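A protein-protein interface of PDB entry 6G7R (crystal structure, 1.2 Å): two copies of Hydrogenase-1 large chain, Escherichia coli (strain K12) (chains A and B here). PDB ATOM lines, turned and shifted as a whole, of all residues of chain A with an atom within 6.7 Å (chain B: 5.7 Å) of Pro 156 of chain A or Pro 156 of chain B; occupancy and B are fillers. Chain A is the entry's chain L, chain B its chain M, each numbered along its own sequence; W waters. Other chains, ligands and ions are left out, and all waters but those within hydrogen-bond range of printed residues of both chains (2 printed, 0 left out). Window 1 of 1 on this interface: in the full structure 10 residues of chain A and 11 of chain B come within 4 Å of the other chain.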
ATOM      1  N   GLN A 150     -24.493  -7.896  -4.005  1.00  0.00           N
ATOM      2  CA  GLN A 150     -25.015  -6.538  -3.895  1.00  0.00           C
ATOM      3  C   GLN A 150     -26.141  -6.300  -4.896  1.00  0.00           C
ATOM      4  O   GLN A 150     -26.985  -5.448  -4.637  1.00  0.00           O
ATOM      5  CB  GLN A 150     -23.884  -5.531  -4.061  1.00  0.00           C
ATOM      6  CG  GLN A 150     -22.916  -5.622  -2.892  1.00  0.00           C
ATOM      7  CD  GLN A 150     -21.682  -4.769  -2.912  1.00  0.00           C
ATOM      8  OE1 GLN A 150     -20.929  -4.761  -1.926  1.00  0.00           O
ATOM      9  NE2 GLN A 150     -21.481  -4.019  -3.975  1.00  0.00           N
ATOM     10  N   SER A 153     -29.384  -8.071  -2.927  1.00  0.00           N
ATOM     11  CA  SER A 153     -29.799  -7.802  -1.564  1.00  0.00           C
ATOM     12  C   SER A 153     -29.121  -6.556  -1.012  1.00  0.00           C
ATOM     13  O   SER A 153     -27.985  -6.215  -1.400  1.00  0.00           O
ATOM     14  CB  SER A 153     -29.463  -8.982  -0.666  1.00  0.00           C
ATOM     15  OG  SER A 153     -29.817  -8.724   0.687  1.00  0.00           O
ATOM     16  N   SER A 154     -29.803  -5.978  -0.031  1.00  0.00           N
ATOM     17  CA  SER A 154     -29.227  -4.890   0.759  1.00  0.00           C
ATOM     18  C   SER A 154     -28.378  -5.427   1.917  1.00  0.00           C
ATOM     19  O   SER A 154     -27.771  -4.621   2.646  1.00  0.00           O
ATOM     20  CB  SER A 154     -30.312  -3.989   1.274  1.00  0.00           C
ATOM     21  OG  SER A 154     -31.199  -4.717   2.107  1.00  0.00           O
ATOM     22  N   TRP A 155     -28.314  -6.748   2.101  1.00  0.00           N
ATOM     23  CA  TRP A 155     -27.593  -7.307   3.250  1.00  0.00           C
ATOM     24  C   TRP A 155     -26.203  -6.674   3.349  1.00  0.00           C
ATOM     25  O   TRP A 155     -25.507  -6.575   2.354  1.00  0.00           O
ATOM     26  CB  TRP A 155     -27.469  -8.819   3.098  1.00  0.00           C
ATOM     27  CG  TRP A 155     -26.862  -9.556   4.244  1.00  0.00           C
ATOM     28  CD1 TRP A 155     -25.783 -10.395   4.227  1.00  0.00           C
ATOM     29  CD2 TRP A 155     -27.420  -9.646   5.563  1.00  0.00           C
ATOM     30  NE1 TRP A 155     -25.610 -10.965   5.464  1.00  0.00           N
ATOM     31  CE2 TRP A 155     -26.607 -10.532   6.302  1.00  0.00           C
ATOM     32  CE3 TRP A 155     -28.533  -9.066   6.181  1.00  0.00           C
ATOM     33  CZ2 TRP A 155     -26.880 -10.833   7.636  1.00  0.00           C
ATOM     34  CZ3 TRP A 155     -28.813  -9.381   7.491  1.00  0.00           C
ATOM     35  CH2 TRP A 155     -27.992 -10.248   8.201  1.00  0.00           C
ATOM     36  N   PRO A 156     -25.772  -6.314   4.566  1.00  0.00           N
ATOM     37  CA  PRO A 156     -24.497  -5.579   4.629  1.00  0.00           C
ATOM     38  C   PRO A 156     -23.265  -6.386   4.217  1.00  0.00           C
ATOM     39  O   PRO A 156     -22.322  -5.798   3.690  1.00  0.00           O
ATOM     40  CB  PRO A 156     -24.388  -5.148   6.100  1.00  0.00           C
ATOM     41  CG  PRO A 156     -25.836  -5.020   6.515  1.00  0.00           C
ATOM     42  CD  PRO A 156     -26.516  -6.166   5.830  1.00  0.00           C
ATOM     43  N   LYS A 157     -23.234  -7.676   4.534  1.00  0.00           N
ATOM     44  CA  LYS A 157     -22.001  -8.449   4.456  1.00  0.00           C
ATOM     45  C   LYS A 157     -21.740  -8.932   3.039  1.00  0.00           C
ATOM     46  O   LYS A 157     -22.163 -10.017   2.642  1.00  0.00           O
ATOM     47  CB  LYS A 157     -22.094  -9.628   5.414  1.00  0.00           C
ATOM     48  CG  LYS A 157     -22.205  -9.210   6.863  1.00  0.00           C
ATOM     49  CD  LYS A 157     -22.123 -10.398   7.778  1.00  0.00           C
ATOM     50  CE  LYS A 157     -22.236 -10.028   9.225  1.00  0.00           C
ATOM     51  NZ  LYS A 157     -22.016 -11.220  10.067  1.00  0.00           N
ATOM     52  N   SER A 158     -21.020  -8.129   2.286  1.00  0.00           N
ATOM     53  CA  SER A 158     -20.906  -8.365   0.856  1.00  0.00           C
ATOM     54  C   SER A 158     -19.546  -7.906   0.332  1.00  0.00           C
ATOM     55  O   SER A 158     -19.382  -7.893  -0.868  1.00  0.00           O
ATOM     56  CB  SER A 158     -21.986  -7.599   0.105  1.00  0.00           C
ATOM     57  OG  SER A 158     -21.741  -6.194   0.269  1.00  0.00           O
ATOM     58  N   SER A 159     -18.581  -7.515   1.164  1.00  0.00           N
ATOM     59  CA  SER A 159     -17.351  -6.956   0.617  1.00  0.00           C
ATOM     60  C   SER A 159     -16.586  -8.033  -0.162  1.00  0.00           C
ATOM     61  O   SER A 159     -16.606  -9.218   0.163  1.00  0.00           O
ATOM     62  CB  SER A 159     -16.483  -6.324   1.688  1.00  0.00           C
ATOM     63  OG  SER A 159     -15.876  -7.325   2.455  1.00  0.00           O
ATOM     64  N   PRO A 160     -15.799  -7.595  -1.144  1.00  0.00           N
ATOM     65  CA  PRO A 160     -14.901  -8.524  -1.832  1.00  0.00           C
ATOM     66  C   PRO A 160     -13.938  -9.192  -0.844  1.00  0.00           C
ATOM     67  O   PRO A 160     -13.628 -10.388  -0.960  1.00  0.00           O
ATOM     68  CB  PRO A 160     -14.096  -7.654  -2.801  1.00  0.00           C
ATOM     69  CG  PRO A 160     -15.029  -6.541  -3.092  1.00  0.00           C
ATOM     70  CD  PRO A 160     -15.758  -6.277  -1.796  1.00  0.00           C
ATOM     71  N   GLY A 161     -13.448  -8.432   0.129  1.00  0.00           N
ATOM     72  CA  GLY A 161     -12.552  -8.982   1.156  1.00  0.00           C
ATOM     73  C   GLY A 161     -13.179 -10.084   1.998  1.00  0.00           C
ATOM     74  O   GLY A 161     -12.532 -11.083   2.364  1.00  0.00           O
ATOM     75  N   TYR A 162     -14.445  -9.909   2.320  1.00  0.00           N
ATOM     76  CA  TYR A 162     -15.204 -10.913   3.029  1.00  0.00           C
ATOM     77  C   TYR A 162     -15.302 -12.203   2.202  1.00  0.00           C
ATOM     78  O   TYR A 162     -15.043 -13.300   2.697  1.00  0.00           O
ATOM     79  CB  TYR A 162     -16.609 -10.393   3.320  1.00  0.00           C
ATOM     80  CG  TYR A 162     -17.583 -11.420   3.842  1.00  0.00           C
ATOM     81  CD1 TYR A 162     -17.336 -12.138   5.000  1.00  0.00           C
ATOM     82  CD2 TYR A 162     -18.794 -11.621   3.209  1.00  0.00           C
ATOM     83  CE1 TYR A 162     -18.260 -13.044   5.483  1.00  0.00           C
ATOM     84  CE2 TYR A 162     -19.723 -12.542   3.668  1.00  0.00           C
ATOM     85  CZ  TYR A 162     -19.465 -13.228   4.835  1.00  0.00           C
ATOM     86  OH  TYR A 162     -20.360 -14.142   5.303  1.00  0.00           O
ATOM     87  N   ASP A 165     -12.034 -13.892   2.133  1.00  0.00           N
ATOM     88  CA  ASP A 165     -11.733 -14.528   3.424  1.00  0.00           C
ATOM     89  C   ASP A 165     -12.502 -15.856   3.537  1.00  0.00           C
ATOM     90  O   ASP A 165     -11.936 -16.876   3.940  1.00  0.00           O
ATOM     91  CB  ASP A 165     -12.034 -13.594   4.606  1.00  0.00           C
ATOM     92  CG  ASP A 165     -11.077 -12.419   4.768  1.00  0.00           C
ATOM     93  OD1 ASP A 165      -9.974 -12.480   4.202  1.00  0.00           O
ATOM     94  OD2 ASP A 165     -11.441 -11.463   5.505  1.00  0.00           O
ATOM     95  N   ASP A 269     -34.765  -9.700   9.848  1.00  0.00           N
ATOM     96  CA  ASP A 269     -33.733  -9.094   9.020  1.00  0.00           C
ATOM     97  C   ASP A 269     -32.963 -10.181   8.260  1.00  0.00           C
ATOM     98  O   ASP A 269     -32.716 -10.074   7.074  1.00  0.00           O
ATOM     99  CB  ASP A 269     -32.825  -8.222   9.893  1.00  0.00           C
ATOM    100  CG  ASP A 269     -31.824  -7.338   9.160  1.00  0.00           C
ATOM    101  OD1 ASP A 269     -32.118  -6.907   8.035  1.00  0.00           O
ATOM    102  OD2 ASP A 269     -30.755  -7.086   9.741  1.00  0.00           O
ATOM    103  N   ASN A 273     -33.353 -10.717   4.144  1.00  0.00           N
ATOM    104  CA  ASN A 273     -32.271 -10.165   3.357  1.00  0.00           C
ATOM    105  C   ASN A 273     -31.206 -11.196   2.974  1.00  0.00           C
ATOM    106  O   ASN A 273     -30.296 -10.902   2.190  1.00  0.00           O
ATOM    107  CB  ASN A 273     -31.657  -8.964   4.080  1.00  0.00           C
ATOM    108  CG  ASN A 273     -32.664  -7.833   4.176  1.00  0.00           C
ATOM    109  OD1 ASN A 273     -33.061  -7.288   3.150  1.00  0.00           O
ATOM    110  ND2 ASN A 273     -33.191  -7.581   5.363  1.00  0.00           N
ATOM    111  N   SER B 154     -11.174  -5.076   4.382  1.00  0.00           N
ATOM    112  CA  SER B 154     -11.860  -6.342   4.105  1.00  0.00           C
ATOM    113  C   SER B 154     -13.134  -6.485   4.947  1.00  0.00           C
ATOM    114  O   SER B 154     -13.860  -7.473   4.785  1.00  0.00           O
ATOM    115  CB  SER B 154     -10.945  -7.527   4.349  1.00  0.00           C
ATOM    116  OG  SER B 154     -10.401  -7.481   5.664  1.00  0.00           O
ATOM    117  N   TRP B 155     -13.419  -5.524   5.817  1.00  0.00           N
ATOM    118  CA  TRP B 155     -14.570  -5.634   6.708  1.00  0.00           C
ATOM    119  C   TRP B 155     -15.822  -6.010   5.922  1.00  0.00           C
ATOM    120  O   TRP B 155     -16.103  -5.414   4.895  1.00  0.00           O
ATOM    121  CB  TRP B 155     -14.803  -4.317   7.448  1.00  0.00           C
ATOM    122  CG  TRP B 155     -15.886  -4.311   8.481  1.00  0.00           C
ATOM    123  CD1 TRP B 155     -16.972  -3.482   8.539  1.00  0.00           C
ATOM    124  CD2 TRP B 155     -15.908  -5.101   9.688  1.00  0.00           C
ATOM    125  NE1 TRP B 155     -17.669  -3.722   9.693  1.00  0.00           N
ATOM    126  CE2 TRP B 155     -17.040  -4.702  10.420  1.00  0.00           C
ATOM    127  CE3 TRP B 155     -15.064  -6.083  10.221  1.00  0.00           C
ATOM    128  CZ2 TRP B 155     -17.359  -5.263  11.662  1.00  0.00           C
ATOM    129  CZ3 TRP B 155     -15.361  -6.618  11.459  1.00  0.00           C
ATOM    130  CH2 TRP B 155     -16.499  -6.215  12.160  1.00  0.00           C
ATOM    131  N   PRO B 156     -16.626  -6.963   6.421  1.00  0.00           N
ATOM    132  CA  PRO B 156     -17.690  -7.434   5.534  1.00  0.00           C
ATOM    133  C   PRO B 156     -18.783  -6.389   5.258  1.00  0.00           C
ATOM    134  O   PRO B 156     -19.346  -6.372   4.159  1.00  0.00           O
ATOM    135  CB  PRO B 156     -18.286  -8.629   6.287  1.00  0.00           C
ATOM    136  CG  PRO B 156     -17.098  -9.197   7.029  1.00  0.00           C
ATOM    137  CD  PRO B 156     -16.359  -7.960   7.475  1.00  0.00           C
ATOM    138  N   LYS B 157     -19.097  -5.547   6.236  1.00  0.00           N
ATOM    139  CA  LYS B 157     -20.331  -4.717   6.228  1.00  0.00           C
ATOM    140  C   LYS B 157     -20.088  -3.459   5.408  1.00  0.00           C
ATOM    141  O   LYS B 157     -19.670  -2.427   5.921  1.00  0.00           O
ATOM    142  CB  LYS B 157     -20.796  -4.411   7.649  1.00  0.00           C
ATOM    143  CG  LYS B 157     -21.236  -5.629   8.441  1.00  0.00           C
ATOM    144  CD  LYS B 157     -21.694  -5.210   9.803  1.00  0.00           C
ATOM    145  CE  LYS B 157     -22.307  -6.321  10.602  1.00  0.00           C
ATOM    146  NZ  LYS B 157     -22.665  -5.801  11.937  1.00  0.00           N
ATOM    147  N   SER B 158     -20.351  -3.568   4.109  1.00  0.00           N
ATOM    148  CA  SER B 158     -19.943  -2.490   3.196  1.00  0.00           C
ATOM    149  C   SER B 158     -20.874  -2.357   1.999  1.00  0.00           C
ATOM    150  O   SER B 158     -20.523  -1.647   1.072  1.00  0.00           O
ATOM    151  CB  SER B 158     -18.555  -2.794   2.677  1.00  0.00           C
ATOM    152  OG  SER B 158     -18.628  -4.010   1.932  1.00  0.00           O
ATOM    153  N   SER B 159     -22.018  -3.030   1.992  1.00  0.00           N
ATOM    154  CA  SER B 159     -22.835  -2.996   0.787  1.00  0.00           C
ATOM    155  C   SER B 159     -23.413  -1.598   0.554  1.00  0.00           C
ATOM    156  O   SER B 159     -23.667  -0.848   1.495  1.00  0.00           O
ATOM    157  CB  SER B 159     -23.954  -3.989   0.843  1.00  0.00           C
ATOM    158  OG  SER B 159     -24.971  -3.601   1.745  1.00  0.00           O
ATOM    159  N   TYR B 162     -26.526  -1.299   2.673  1.00  0.00           N
ATOM    160  CA  TYR B 162     -26.214  -1.002   4.057  1.00  0.00           C
ATOM    161  C   TYR B 162     -26.016   0.500   4.259  1.00  0.00           C
ATOM    162  O   TYR B 162     -26.618   1.105   5.158  1.00  0.00           O
ATOM    163  CB  TYR B 162     -24.968  -1.776   4.478  1.00  0.00           C
ATOM    164  CG  TYR B 162     -24.394  -1.399   5.819  1.00  0.00           C
ATOM    165  CD1 TYR B 162     -25.142  -1.491   6.977  1.00  0.00           C
ATOM    166  CD2 TYR B 162     -23.101  -0.922   5.922  1.00  0.00           C
ATOM    167  CE1 TYR B 162     -24.580  -1.201   8.206  1.00  0.00           C
ATOM    168  CE2 TYR B 162     -22.542  -0.586   7.143  1.00  0.00           C
ATOM    169  CZ  TYR B 162     -23.281  -0.739   8.289  1.00  0.00           C
ATOM    170  OH  TYR B 162     -22.745  -0.399   9.494  1.00  0.00           O
HETATM  171  O   HOH W   1     -10.587  -9.468   7.140  1.00  0.00           O
HETATM  172  O   HOH W   2     -13.606 -10.048   5.970  1.00  0.00           O
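Water W1 bridges the side-chain hydroxyl of Ser 154 of chain B (2.5 Å) and the side-chain carboxylate of Asp 165 of chain A (2.7 Å). Water W2 bridges OD2 of Asp 165 of chain A (2.6 Å) and O of Ser 154 of chain B (2.8 Å).
OE1 of Gln 150 of chain A touches CA of Ser 159 of chain B, at 3.8 Å. Ser 154 of chain A touches Tyr 162 of chain B. Pro 156 of chain A touches Lys 157 of chain B (O to CA, 3.4 Å). CG of Pro 156 of chain A touches CD1 of Tyr 162 of chain B (3.6 Å). Lys 157 of chain A touches Pro 156 of chain B. Lys 157 of chain A touches Lys 157 of chain B (CE to CE, 3.96 Å). Ser 159 of chain A touches Ser 158 of chain B (CB to OG, 3.2 Å). Gly 161 of chain A touches Ser 154 of chain B. Tyr 162 of chain A touches Ser 154 of chain B. Tyr 162 of chain A touches Pro 156 of chain B (CD1 to CG, 3.6 Å).
The backbone NH (N) of Ser 159 of chain A is in hydrogen-bond range of the backbone carbonyl oxygen (O) of Pro 156 of chain B (3.3 Å). O of Pro 156 of chain B sits close to O of Pro 156 of chain A (3.1 Å). The backbone carbonyl oxygen (O) of Trp 155 of chain B lies within hydrogen-bond range of the side-chain hydroxyl (OG) of Ser 159 of chain A, 3.1 Å away. O of Trp 155 of chain A sits at hydrogen-bond distance from OG of Ser 159 of chain B (3.1 Å). OG of Ser 159 of chain B is in hydrogen-bond range of O of Ser 154 of chain A (3.1 Å). The backbone carbonyl oxygen (O) of Pro 156 of chain A is in hydrogen-bond range of the backbone NH (N) of Ser 159 of chain B (3.3 Å). The backbone carbonyl oxygen (O) of Pro 156 of chain A sits at hydrogen-bond distance from the backbone NH (N) of Ser 158 of chain B, at 3.0 Å. OG of Ser 159 of chain A sits at hydrogen-bond distance from O of Ser 154 of chain B (3.1 Å). O of Pro 156 of chain B is in hydrogen-bond range of N of Ser 158 of chain A, at 3.1 Å.
Ser 154 of chain A touches Tyr 162 of chain B, and with the chains exchanged Tyr 162 of chain A touches Ser 154 of chain B. Pro 156 of chain A touches Ser 158 of chain B, and with the chains exchanged Ser 158 of chain A touches Pro 156 of chain B. Pro 156 of chain A touches Ser 159 of chain B, and with the chains exchanged Ser 159 of chain A touches Pro 156 of chain B. Lys 157 of chain A touches its own counterpart, Lys 157 of chain B. Positions printed for both chains: 154, 155, 156, 157, 158, 159 and 162.
Hydrophobic or aromatic side chains of chain A within 4 Å of the printed part of chain B: Pro 156 and Tyr 162. Along chain A the printed residues that touch a printed residue of chain B span positions 150 to 162. Among the printed residues, no Asp or Glu carboxylate lies within 4 Å of a Lys or Arg side-chain nitrogen of the other chain.
The backbone carbonyl oxygen of Pro 156 of chain A is in hydrogen-bond range of the side-chain hydroxyl of Ser 158 of chain A (3.5 Å). N of Tyr 162 of chain B sits at hydrogen-bond distance from OG of Ser 159 of chain B, at 2.9 Å. The side-chain hydroxyl of Ser 159 of chain A lies within hydrogen-bond range of the backbone NH of Tyr 162 of chain A (3.0 Å). O of Pro 156 of chain B lies within hydrogen-bond range of OG of Ser 158 of chain B (3.3 Å). The backbone NH (N) of Trp 155 of chain A lies within hydrogen-bond range of the side-chain hydroxyl (OG) of Ser 153 of chain A (2.9 Å). The side-chain hydroxyl (OG) of Ser 158 of chain A sits at hydrogen-bond distance from the side-chain amide oxygen (OE1) of Gln 150 of chain A (2.7 Å).
Of chain B, only Pro 156 (3.1 Å), Lys 157 (3.4 Å), Ser 158 (3.0 Å), Ser 159 (3.3 Å) and Tyr 162 (3.6 Å) come within 4 Å of Pro 156 of chain A. Pro 156 of chain B touches just these residues of chain A: Pro 156 (3.1 Å), Lys 157 (3.4 Å), Ser 158 (3.1 Å), Ser 159 (3.3 Å) and Tyr 162 (3.6 Å). Printed residues of chain A within 4 Å of Lys 157 of chain B: Pro 156 and Lys 157. Of the printed residues of chain A, Tyr 162 of chain B touches Ser 154 (3.5 Å) and Pro 156 (3.6 Å). Of the printed residues of chain A, Ser 154 of chain B touches Ser 159 (3.1 Å), Gly 161 (3.9 Å) and Tyr 162 (3.5 Å). Ser 153 of chain A touches none of the printed residues of chain B. The nearest printed residue of chain B that does not touch Pro 156 of chain A is Trp 155 of chain B (6.3 Å). The nearest printed residue of chain A that does not touch Pro 156 of chain B is Asp 165 of chain A (6.3 Å).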
